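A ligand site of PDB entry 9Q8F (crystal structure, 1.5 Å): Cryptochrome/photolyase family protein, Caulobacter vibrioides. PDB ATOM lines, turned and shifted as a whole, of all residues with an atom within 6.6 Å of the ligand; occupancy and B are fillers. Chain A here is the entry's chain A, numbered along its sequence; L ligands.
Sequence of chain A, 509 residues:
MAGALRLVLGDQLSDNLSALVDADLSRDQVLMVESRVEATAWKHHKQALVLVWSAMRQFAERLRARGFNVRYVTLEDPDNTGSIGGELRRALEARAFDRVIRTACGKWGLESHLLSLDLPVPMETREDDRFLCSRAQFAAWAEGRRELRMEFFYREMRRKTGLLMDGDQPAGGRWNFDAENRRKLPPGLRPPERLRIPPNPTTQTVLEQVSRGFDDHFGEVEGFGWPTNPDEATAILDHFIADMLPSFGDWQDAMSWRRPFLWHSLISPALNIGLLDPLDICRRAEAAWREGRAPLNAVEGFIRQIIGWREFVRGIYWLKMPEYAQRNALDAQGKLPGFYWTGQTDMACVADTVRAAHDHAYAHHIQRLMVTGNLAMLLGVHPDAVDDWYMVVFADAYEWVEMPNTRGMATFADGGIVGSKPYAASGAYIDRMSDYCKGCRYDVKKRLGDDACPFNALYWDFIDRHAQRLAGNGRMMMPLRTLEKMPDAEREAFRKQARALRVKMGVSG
The side-chain sulfur of Cys 453 is bound to an iron atom (FE2) of the ligand, at 2.3 Å. An iron atom (FE4) of the ligand is bound by the side-chain sulfur of Cys 440 (2.3 Å). The side-chain sulfur (SG) of Cys 437 is bound to an iron atom (FE1) of the ligand, 2.3 Å away. N of Cys 349 sits close to S2 of the ligand, 3.6 Å away. SG of Cys 349 is bound to FE3 of the ligand (2.3 Å).
SG of Cys 453 sits close to N of Phe 455 (3.5 Å). The backbone NH of Cys 453 sits at hydrogen-bond distance from the backbone carbonyl oxygen of Asp 443. The side-chain sulfur of Cys 440 sits close to the backbone NH of Tyr 442. The backbone NH (N) of Ala 348 lies close to the side-chain sulfur (SG) of Cys 440 (3.6 Å). N of Tyr 436 lies within hydrogen-bond range of OG of Ser 434 (3.0 Å). The backbone carbonyl oxygen (O) of Ile 430 is in hydrogen-bond range of the side-chain hydroxyl (OG) of Ser 434, 2.7 Å away. The backbone carbonyl oxygen of Val 444 sits at hydrogen-bond distance from the side-chain amide nitrogen of Asn 456 (3.0 Å). The backbone NH (N) of Gly 427 lies within hydrogen-bond range of the side-chain amide oxygen (OD1) of Asn 456 (2.9 Å).
Merely in contact with the ligand: Tyr 436 (3.5 Å), Met 347 (3.5 Å), Ile 430 (3.6 Å), Val 444 (3.7 Å), Gly 427 (3.9 Å), Tyr 442 (3.9 Å) and Ala 348 (3.96 Å). Hydrophobic or aromatic side chains that line the ligand: Met 347, Ala 348, Ile 430, Tyr 436 and Val 444. Of the 26 residues printed, 11 come within 4 Å of the ligand. The nearest printed residue that does not touch the ligand is Phe 455 (4.2 Å).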
ATOM      1  N   ASP A 346     -20.366 -14.465 -16.914  1.00  0.00           N
ATOM      2  CA  ASP A 346     -20.352 -15.147 -15.631  1.00  0.00           C
ATOM      3  C   ASP A 346     -19.009 -15.044 -14.907  1.00  0.00           C
ATOM      4  O   ASP A 346     -18.911 -15.549 -13.781  1.00  0.00           O
ATOM      5  CB  ASP A 346     -20.700 -16.630 -15.822  1.00  0.00           C
ATOM      6  CG  ASP A 346     -22.197 -16.871 -15.924  1.00  0.00           C
ATOM      7  OD1 ASP A 346     -22.987 -15.950 -15.672  1.00  0.00           O
ATOM      8  OD2 ASP A 346     -22.553 -18.001 -16.305  1.00  0.00           O
ATOM      9  N   MET A 347     -17.979 -14.433 -15.490  1.00  0.00           N
ATOM     10  CA  MET A 347     -16.751 -14.170 -14.762  1.00  0.00           C
ATOM     11  C   MET A 347     -17.009 -13.004 -13.810  1.00  0.00           C
ATOM     12  O   MET A 347     -17.123 -11.856 -14.247  1.00  0.00           O
ATOM     13  CB  MET A 347     -15.602 -13.867 -15.704  1.00  0.00           C
ATOM     14  CG  MET A 347     -15.294 -14.969 -16.708  1.00  0.00           C
ATOM     15  SD  MET A 347     -13.848 -14.633 -17.730  1.00  0.00           S
ATOM     16  CE  MET A 347     -14.669 -13.717 -19.013  1.00  0.00           C
ATOM     17  N   ALA A 348     -17.088 -13.297 -12.515  1.00  0.00           N
ATOM     18  CA  ALA A 348     -17.557 -12.307 -11.554  1.00  0.00           C
ATOM     19  C   ALA A 348     -16.625 -11.098 -11.492  1.00  0.00           C
ATOM     20  O   ALA A 348     -17.089  -9.961 -11.382  1.00  0.00           O
ATOM     21  CB  ALA A 348     -17.685 -12.950 -10.175  1.00  0.00           C
ATOM     22  N   CYS A 349     -15.320 -11.349 -11.562  1.00  0.00           N
ATOM     23  CA  CYS A 349     -14.328 -10.280 -11.512  1.00  0.00           C
ATOM     24  C   CYS A 349     -14.487  -9.326 -12.692  1.00  0.00           C
ATOM     25  O   CYS A 349     -14.450  -8.089 -12.535  1.00  0.00           O
ATOM     26  CB  CYS A 349     -12.925 -10.883 -11.485  1.00  0.00           C
ATOM     27  SG  CYS A 349     -12.590 -12.130 -12.822  1.00  0.00           S
ATOM     28  N   VAL A 350     -14.619  -9.887 -13.898  1.00  0.00           N
ATOM     29  CA  VAL A 350     -14.782  -9.076 -15.101  1.00  0.00           C
ATOM     30  C   VAL A 350     -16.090  -8.303 -15.054  1.00  0.00           C
ATOM     31  O   VAL A 350     -16.143  -7.097 -15.334  1.00  0.00           O
ATOM     32  CB  VAL A 350     -14.707  -9.981 -16.347  1.00  0.00           C
ATOM     33  CG1 VAL A 350     -15.008  -9.166 -17.569  1.00  0.00           C
ATOM     34  CG2 VAL A 350     -13.331 -10.645 -16.460  1.00  0.00           C
ATOM     35  N   VAL A 371      -7.394  -7.674 -14.171  1.00  0.00           N
ATOM     36  CA  VAL A 371      -8.653  -8.304 -14.553  1.00  0.00           C
ATOM     37  C   VAL A 371      -8.880  -8.056 -16.046  1.00  0.00           C
ATOM     38  O   VAL A 371      -8.598  -8.946 -16.859  1.00  0.00           O
ATOM     39  CB  VAL A 371      -9.836  -7.825 -13.691  1.00  0.00           C
ATOM     40  CG1 VAL A 371     -11.079  -8.512 -14.088  1.00  0.00           C
ATOM     41  CG2 VAL A 371      -9.545  -8.141 -12.215  1.00  0.00           C
ATOM     42  N   SER A 426      -3.045 -16.073 -13.843  1.00  0.00           N
ATOM     43  CA  SER A 426      -4.185 -16.971 -13.816  1.00  0.00           C
ATOM     44  C   SER A 426      -5.202 -16.505 -12.781  1.00  0.00           C
ATOM     45  O   SER A 426      -5.030 -15.486 -12.102  1.00  0.00           O
ATOM     46  CB  SER A 426      -3.729 -18.402 -13.507  1.00  0.00           C
ATOM     47  OG  SER A 426      -3.352 -18.482 -12.138  1.00  0.00           O
ATOM     48  N   GLY A 427      -6.288 -17.273 -12.666  1.00  0.00           N
ATOM     49  CA  GLY A 427      -7.293 -16.978 -11.659  1.00  0.00           C
ATOM     50  C   GLY A 427      -6.766 -17.049 -10.245  1.00  0.00           C
ATOM     51  O   GLY A 427      -7.320 -16.411  -9.351  1.00  0.00           O
ATOM     52  N   ALA A 428      -5.676 -17.795 -10.021  1.00  0.00           N
ATOM     53  CA  ALA A 428      -5.106 -17.865  -8.675  1.00  0.00           C
ATOM     54  C   ALA A 428      -4.703 -16.496  -8.153  1.00  0.00           C
ATOM     55  O   ALA A 428      -4.806 -16.238  -6.950  1.00  0.00           O
ATOM     56  CB  ALA A 428      -3.895 -18.803  -8.672  1.00  0.00           C
ATOM     57  N   ILE A 430      -6.157 -13.533  -8.958  1.00  0.00           N
ATOM     58  CA  ILE A 430      -7.387 -12.839  -8.607  1.00  0.00           C
ATOM     59  C   ILE A 430      -7.974 -13.419  -7.319  1.00  0.00           C
ATOM     60  O   ILE A 430      -8.474 -12.666  -6.473  1.00  0.00           O
ATOM     61  CB  ILE A 430      -8.377 -12.912  -9.801  1.00  0.00           C
ATOM     62  CG1 ILE A 430      -7.818 -12.077 -10.967  1.00  0.00           C
ATOM     63  CG2 ILE A 430      -9.740 -12.389  -9.402  1.00  0.00           C
ATOM     64  CD1 ILE A 430      -8.558 -12.246 -12.298  1.00  0.00           C
ATOM     65  N   ASP A 431      -7.890 -14.737  -7.138  1.00  0.00           N
ATOM     66  CA  ASP A 431      -8.392 -15.358  -5.904  1.00  0.00           C
ATOM     67  C   ASP A 431      -7.627 -14.852  -4.687  1.00  0.00           C
ATOM     68  O   ASP A 431      -8.232 -14.527  -3.655  1.00  0.00           O
ATOM     69  CB  ASP A 431      -8.273 -16.882  -6.021  1.00  0.00           C
ATOM     70  CG  ASP A 431      -8.948 -17.627  -4.902  1.00  0.00           C
ATOM     71  OD1 ASP A 431      -9.928 -17.126  -4.296  1.00  0.00           O
ATOM     72  OD2 ASP A 431      -8.498 -18.762  -4.610  1.00  0.00           O
ATOM     73  N   SER A 434      -8.548 -10.877  -4.087  1.00  0.00           N
ATOM     74  CA  SER A 434      -9.939 -10.445  -4.120  1.00  0.00           C
ATOM     75  C   SER A 434     -10.842 -11.386  -3.332  1.00  0.00           C
ATOM     76  O   SER A 434     -10.450 -12.496  -2.942  1.00  0.00           O
ATOM     77  CB  SER A 434     -10.478 -10.385  -5.561  1.00  0.00           C
ATOM     78  OG  SER A 434     -10.924 -11.686  -5.963  1.00  0.00           O
ATOM     79  N   TYR A 436     -13.696 -12.290  -5.018  1.00  0.00           N
ATOM     80  CA  TYR A 436     -14.591 -12.613  -6.121  1.00  0.00           C
ATOM     81  C   TYR A 436     -14.909 -14.103  -6.238  1.00  0.00           C
ATOM     82  O   TYR A 436     -16.039 -14.464  -6.569  1.00  0.00           O
ATOM     83  CB  TYR A 436     -13.989 -12.161  -7.453  1.00  0.00           C
ATOM     84  CG  TYR A 436     -14.017 -10.696  -7.707  1.00  0.00           C
ATOM     85  CD1 TYR A 436     -15.206  -9.970  -7.651  1.00  0.00           C
ATOM     86  CD2 TYR A 436     -12.854 -10.036  -8.047  1.00  0.00           C
ATOM     87  CE1 TYR A 436     -15.223  -8.626  -7.892  1.00  0.00           C
ATOM     88  CE2 TYR A 436     -12.865  -8.659  -8.305  1.00  0.00           C
ATOM     89  CZ  TYR A 436     -14.053  -7.976  -8.223  1.00  0.00           C
ATOM     90  OH  TYR A 436     -14.138  -6.614  -8.475  1.00  0.00           O
ATOM     91  N   CYS A 437     -13.908 -14.978  -6.060  1.00  0.00           N
ATOM     92  CA  CYS A 437     -14.025 -16.318  -6.621  1.00  0.00           C
ATOM     93  C   CYS A 437     -14.991 -17.220  -5.848  1.00  0.00           C
ATOM     94  O   CYS A 437     -15.564 -18.141  -6.435  1.00  0.00           O
ATOM     95  CB  CYS A 437     -12.636 -16.950  -6.698  1.00  0.00           C
ATOM     96  SG  CYS A 437     -11.435 -16.042  -7.697  1.00  0.00           S
ATOM     97  N   LYS A 438     -15.197 -16.977  -4.544  1.00  0.00           N
ATOM     98  CA  LYS A 438     -16.105 -17.827  -3.771  1.00  0.00           C
ATOM     99  C   LYS A 438     -17.501 -17.813  -4.373  1.00  0.00           C
ATOM    100  O   LYS A 438     -18.152 -18.860  -4.492  1.00  0.00           O
ATOM    101  CB  LYS A 438     -16.144 -17.383  -2.309  1.00  0.00           C
ATOM    102  N   CYS A 440     -18.272 -16.835  -7.486  1.00  0.00           N
ATOM    103  CA  CYS A 440     -18.271 -16.940  -8.940  1.00  0.00           C
ATOM    104  C   CYS A 440     -18.860 -18.278  -9.389  1.00  0.00           C
ATOM    105  O   CYS A 440     -18.724 -19.309  -8.711  1.00  0.00           O
ATOM    106  CB  CYS A 440     -16.839 -16.790  -9.466  1.00  0.00           C
ATOM    107  SG  CYS A 440     -16.723 -16.693 -11.289  1.00  0.00           S
ATOM    108  N   ARG A 441     -19.509 -18.252 -10.554  1.00  0.00           N
ATOM    109  CA  ARG A 441     -19.978 -19.466 -11.199  1.00  0.00           C
ATOM    110  C   ARG A 441     -18.841 -20.437 -11.494  1.00  0.00           C
ATOM    111  O   ARG A 441     -19.017 -21.661 -11.432  1.00  0.00           O
ATOM    112  CB  ARG A 441     -20.697 -19.091 -12.499  1.00  0.00           C
ATOM    113  CG  ARG A 441     -21.086 -20.258 -13.404  1.00  0.00           C
ATOM    114  CD  ARG A 441     -20.256 -20.263 -14.678  1.00  0.00           C
ATOM    115  NE  ARG A 441     -20.616 -21.331 -15.594  1.00  0.00           N
ATOM    116  CZ  ARG A 441     -20.382 -22.620 -15.381  1.00  0.00           C
ATOM    117  NH1 ARG A 441     -19.847 -23.056 -14.252  1.00  0.00           N
ATOM    118  NH2 ARG A 441     -20.715 -23.508 -16.323  1.00  0.00           N
ATOM    119  N   TYR A 442     -17.663 -19.917 -11.844  1.00  0.00           N
ATOM    120  CA  TYR A 442     -16.534 -20.744 -12.224  1.00  0.00           C
ATOM    121  C   TYR A 442     -15.751 -21.195 -10.987  1.00  0.00           C
ATOM    122  O   TYR A 442     -15.810 -20.586  -9.921  1.00  0.00           O
ATOM    123  CB  TYR A 442     -15.587 -19.992 -13.158  1.00  0.00           C
ATOM    124  CG  TYR A 442     -16.199 -19.675 -14.499  1.00  0.00           C
ATOM    125  CD1 TYR A 442     -16.351 -20.669 -15.472  1.00  0.00           C
ATOM    126  CD2 TYR A 442     -16.638 -18.395 -14.796  1.00  0.00           C
ATOM    127  CE1 TYR A 442     -16.908 -20.365 -16.717  1.00  0.00           C
ATOM    128  CE2 TYR A 442     -17.201 -18.083 -16.026  1.00  0.00           C
ATOM    129  CZ  TYR A 442     -17.333 -19.082 -16.987  1.00  0.00           C
ATOM    130  OH  TYR A 442     -17.895 -18.751 -18.186  1.00  0.00           O
ATOM    131  N   ASP A 443     -14.960 -22.241 -11.185  1.00  0.00           N
ATOM    132  CA  ASP A 443     -14.157 -22.854 -10.128  1.00  0.00           C
ATOM    133  C   ASP A 443     -12.689 -22.493 -10.371  1.00  0.00           C
ATOM    134  O   ASP A 443     -12.062 -23.023 -11.298  1.00  0.00           O
ATOM    135  CB  ASP A 443     -14.386 -24.362 -10.132  1.00  0.00           C
ATOM    136  CG  ASP A 443     -13.712 -25.067  -8.967  1.00  0.00           C
ATOM    137  OD1 ASP A 443     -14.124 -26.206  -8.640  1.00  0.00           O
ATOM    138  OD2 ASP A 443     -12.824 -24.471  -8.343  1.00  0.00           O
ATOM    139  N   VAL A 444     -12.143 -21.609  -9.529  1.00  0.00           N
ATOM    140  CA  VAL A 444     -10.772 -21.126  -9.729  1.00  0.00           C
ATOM    141  C   VAL A 444      -9.736 -22.203  -9.443  1.00  0.00           C
ATOM    142  O   VAL A 444      -8.552 -22.019  -9.772  1.00  0.00           O
ATOM    143  CB  VAL A 444     -10.533 -19.876  -8.852  1.00  0.00           C
ATOM    144  CG1 VAL A 444     -10.350 -20.245  -7.384  1.00  0.00           C
ATOM    145  CG2 VAL A 444      -9.338 -19.060  -9.367  1.00  0.00           C
ATOM    146  N   LYS A 445     -10.153 -23.332  -8.886  1.00  0.00           N
ATOM    147  CA  LYS A 445      -9.248 -24.443  -8.665  1.00  0.00           C
ATOM    148  C   LYS A 445      -9.166 -25.379  -9.867  1.00  0.00           C
ATOM    149  O   LYS A 445      -8.398 -26.358  -9.820  1.00  0.00           O
ATOM    150  CB  LYS A 445      -9.672 -25.243  -7.425  1.00  0.00           C
ATOM    151  CG  LYS A 445      -9.583 -24.459  -6.121  1.00  0.00           C
ATOM    152  CD  LYS A 445      -8.232 -23.791  -5.960  1.00  0.00           C
ATOM    153  CE  LYS A 445      -7.961 -23.416  -4.510  1.00  0.00           C
ATOM    154  NZ  LYS A 445      -6.672 -22.689  -4.354  1.00  0.00           N
ATOM    155  N   ALA A 452     -14.366 -24.551 -15.269  1.00  0.00           N
ATOM    156  CA  ALA A 452     -13.065 -23.981 -14.940  1.00  0.00           C
ATOM    157  C   ALA A 452     -13.036 -22.475 -15.159  1.00  0.00           C
ATOM    158  O   ALA A 452     -13.515 -21.971 -16.175  1.00  0.00           O
ATOM    159  CB  ALA A 452     -11.975 -24.624 -15.787  1.00  0.00           C
ATOM    160  N   CYS A 453     -12.402 -21.770 -14.227  1.00  0.00           N
ATOM    161  CA  CYS A 453     -12.107 -20.355 -14.399  1.00  0.00           C
ATOM    162  C   CYS A 453     -11.393 -20.135 -15.729  1.00  0.00           C
ATOM    163  O   CYS A 453     -10.319 -20.723 -15.960  1.00  0.00           O
ATOM    164  CB  CYS A 453     -11.238 -19.876 -13.236  1.00  0.00           C
ATOM    165  SG  CYS A 453     -10.524 -18.219 -13.475  1.00  0.00           S
ATOM    166  N   PRO A 454     -11.942 -19.322 -16.639  1.00  0.00           N
ATOM    167  CA  PRO A 454     -11.272 -19.154 -17.942  1.00  0.00           C
ATOM    168  C   PRO A 454      -9.842 -18.630 -17.847  1.00  0.00           C
ATOM    169  O   PRO A 454      -9.029 -18.930 -18.719  1.00  0.00           O
ATOM    170  CB  PRO A 454     -12.190 -18.167 -18.692  1.00  0.00           C
ATOM    171  CG  PRO A 454     -13.540 -18.425 -18.123  1.00  0.00           C
ATOM    172  CD  PRO A 454     -13.285 -18.718 -16.640  1.00  0.00           C
ATOM    173  N   PHE A 455      -9.513 -17.807 -16.831  1.00  0.00           N
ATOM    174  CA  PHE A 455      -8.154 -17.277 -16.756  1.00  0.00           C
ATOM    175  C   PHE A 455      -7.102 -18.384 -16.646  1.00  0.00           C
ATOM    176  O   PHE A 455      -5.944 -18.173 -17.032  1.00  0.00           O
ATOM    177  CB  PHE A 455      -8.000 -16.334 -15.542  1.00  0.00           C
ATOM    178  CG  PHE A 455      -8.641 -14.967 -15.705  1.00  0.00           C
ATOM    179  CD1 PHE A 455      -9.982 -14.783 -15.407  1.00  0.00           C
ATOM    180  CD2 PHE A 455      -7.881 -13.858 -16.044  1.00  0.00           C
ATOM    181  CE1 PHE A 455     -10.564 -13.539 -15.513  1.00  0.00           C
ATOM    182  CE2 PHE A 455      -8.458 -12.614 -16.141  1.00  0.00           C
ATOM    183  CZ  PHE A 455      -9.805 -12.451 -15.862  1.00  0.00           C
ATOM    184  N   ASN A 456      -7.465 -19.561 -16.137  1.00  0.00           N
ATOM    185  CA  ASN A 456      -6.460 -20.574 -15.817  1.00  0.00           C
ATOM    186  C   ASN A 456      -5.900 -21.196 -17.077  1.00  0.00           C
ATOM    187  O   ASN A 456      -4.673 -21.233 -17.267  1.00  0.00           O
ATOM    188  CB  ASN A 456      -7.048 -21.630 -14.881  1.00  0.00           C
ATOM    189  CG  ASN A 456      -7.218 -21.109 -13.457  1.00  0.00           C
ATOM    190  OD1 ASN A 456      -6.616 -20.123 -13.070  1.00  0.00           O
ATOM    191  ND2 ASN A 456      -8.072 -21.753 -12.692  1.00  0.00           N
HETATM  192 FE1  LIG L   1     -12.280 -15.905  -9.820  1.00  0.00          FE
HETATM  193 FE2  LIG L   1     -11.974 -16.897 -12.325  1.00  0.00          FE
HETATM  194 FE3  LIG L   1     -12.690 -14.258 -11.968  1.00  0.00          FE
HETATM  195 FE4  LIG L   1     -14.494 -16.271 -11.472  1.00  0.00          FE
HETATM  196  S1  LIG L   1     -13.604 -15.763 -13.491  1.00  0.00           S
HETATM  197  S2  LIG L   1     -14.011 -14.427 -10.152  1.00  0.00           S
HETATM  198  S3  LIG L   1     -13.094 -17.907 -10.660  1.00  0.00           S
HETATM  199  S4  LIG L   1     -10.740 -15.255 -11.309  1.00  0.00           S
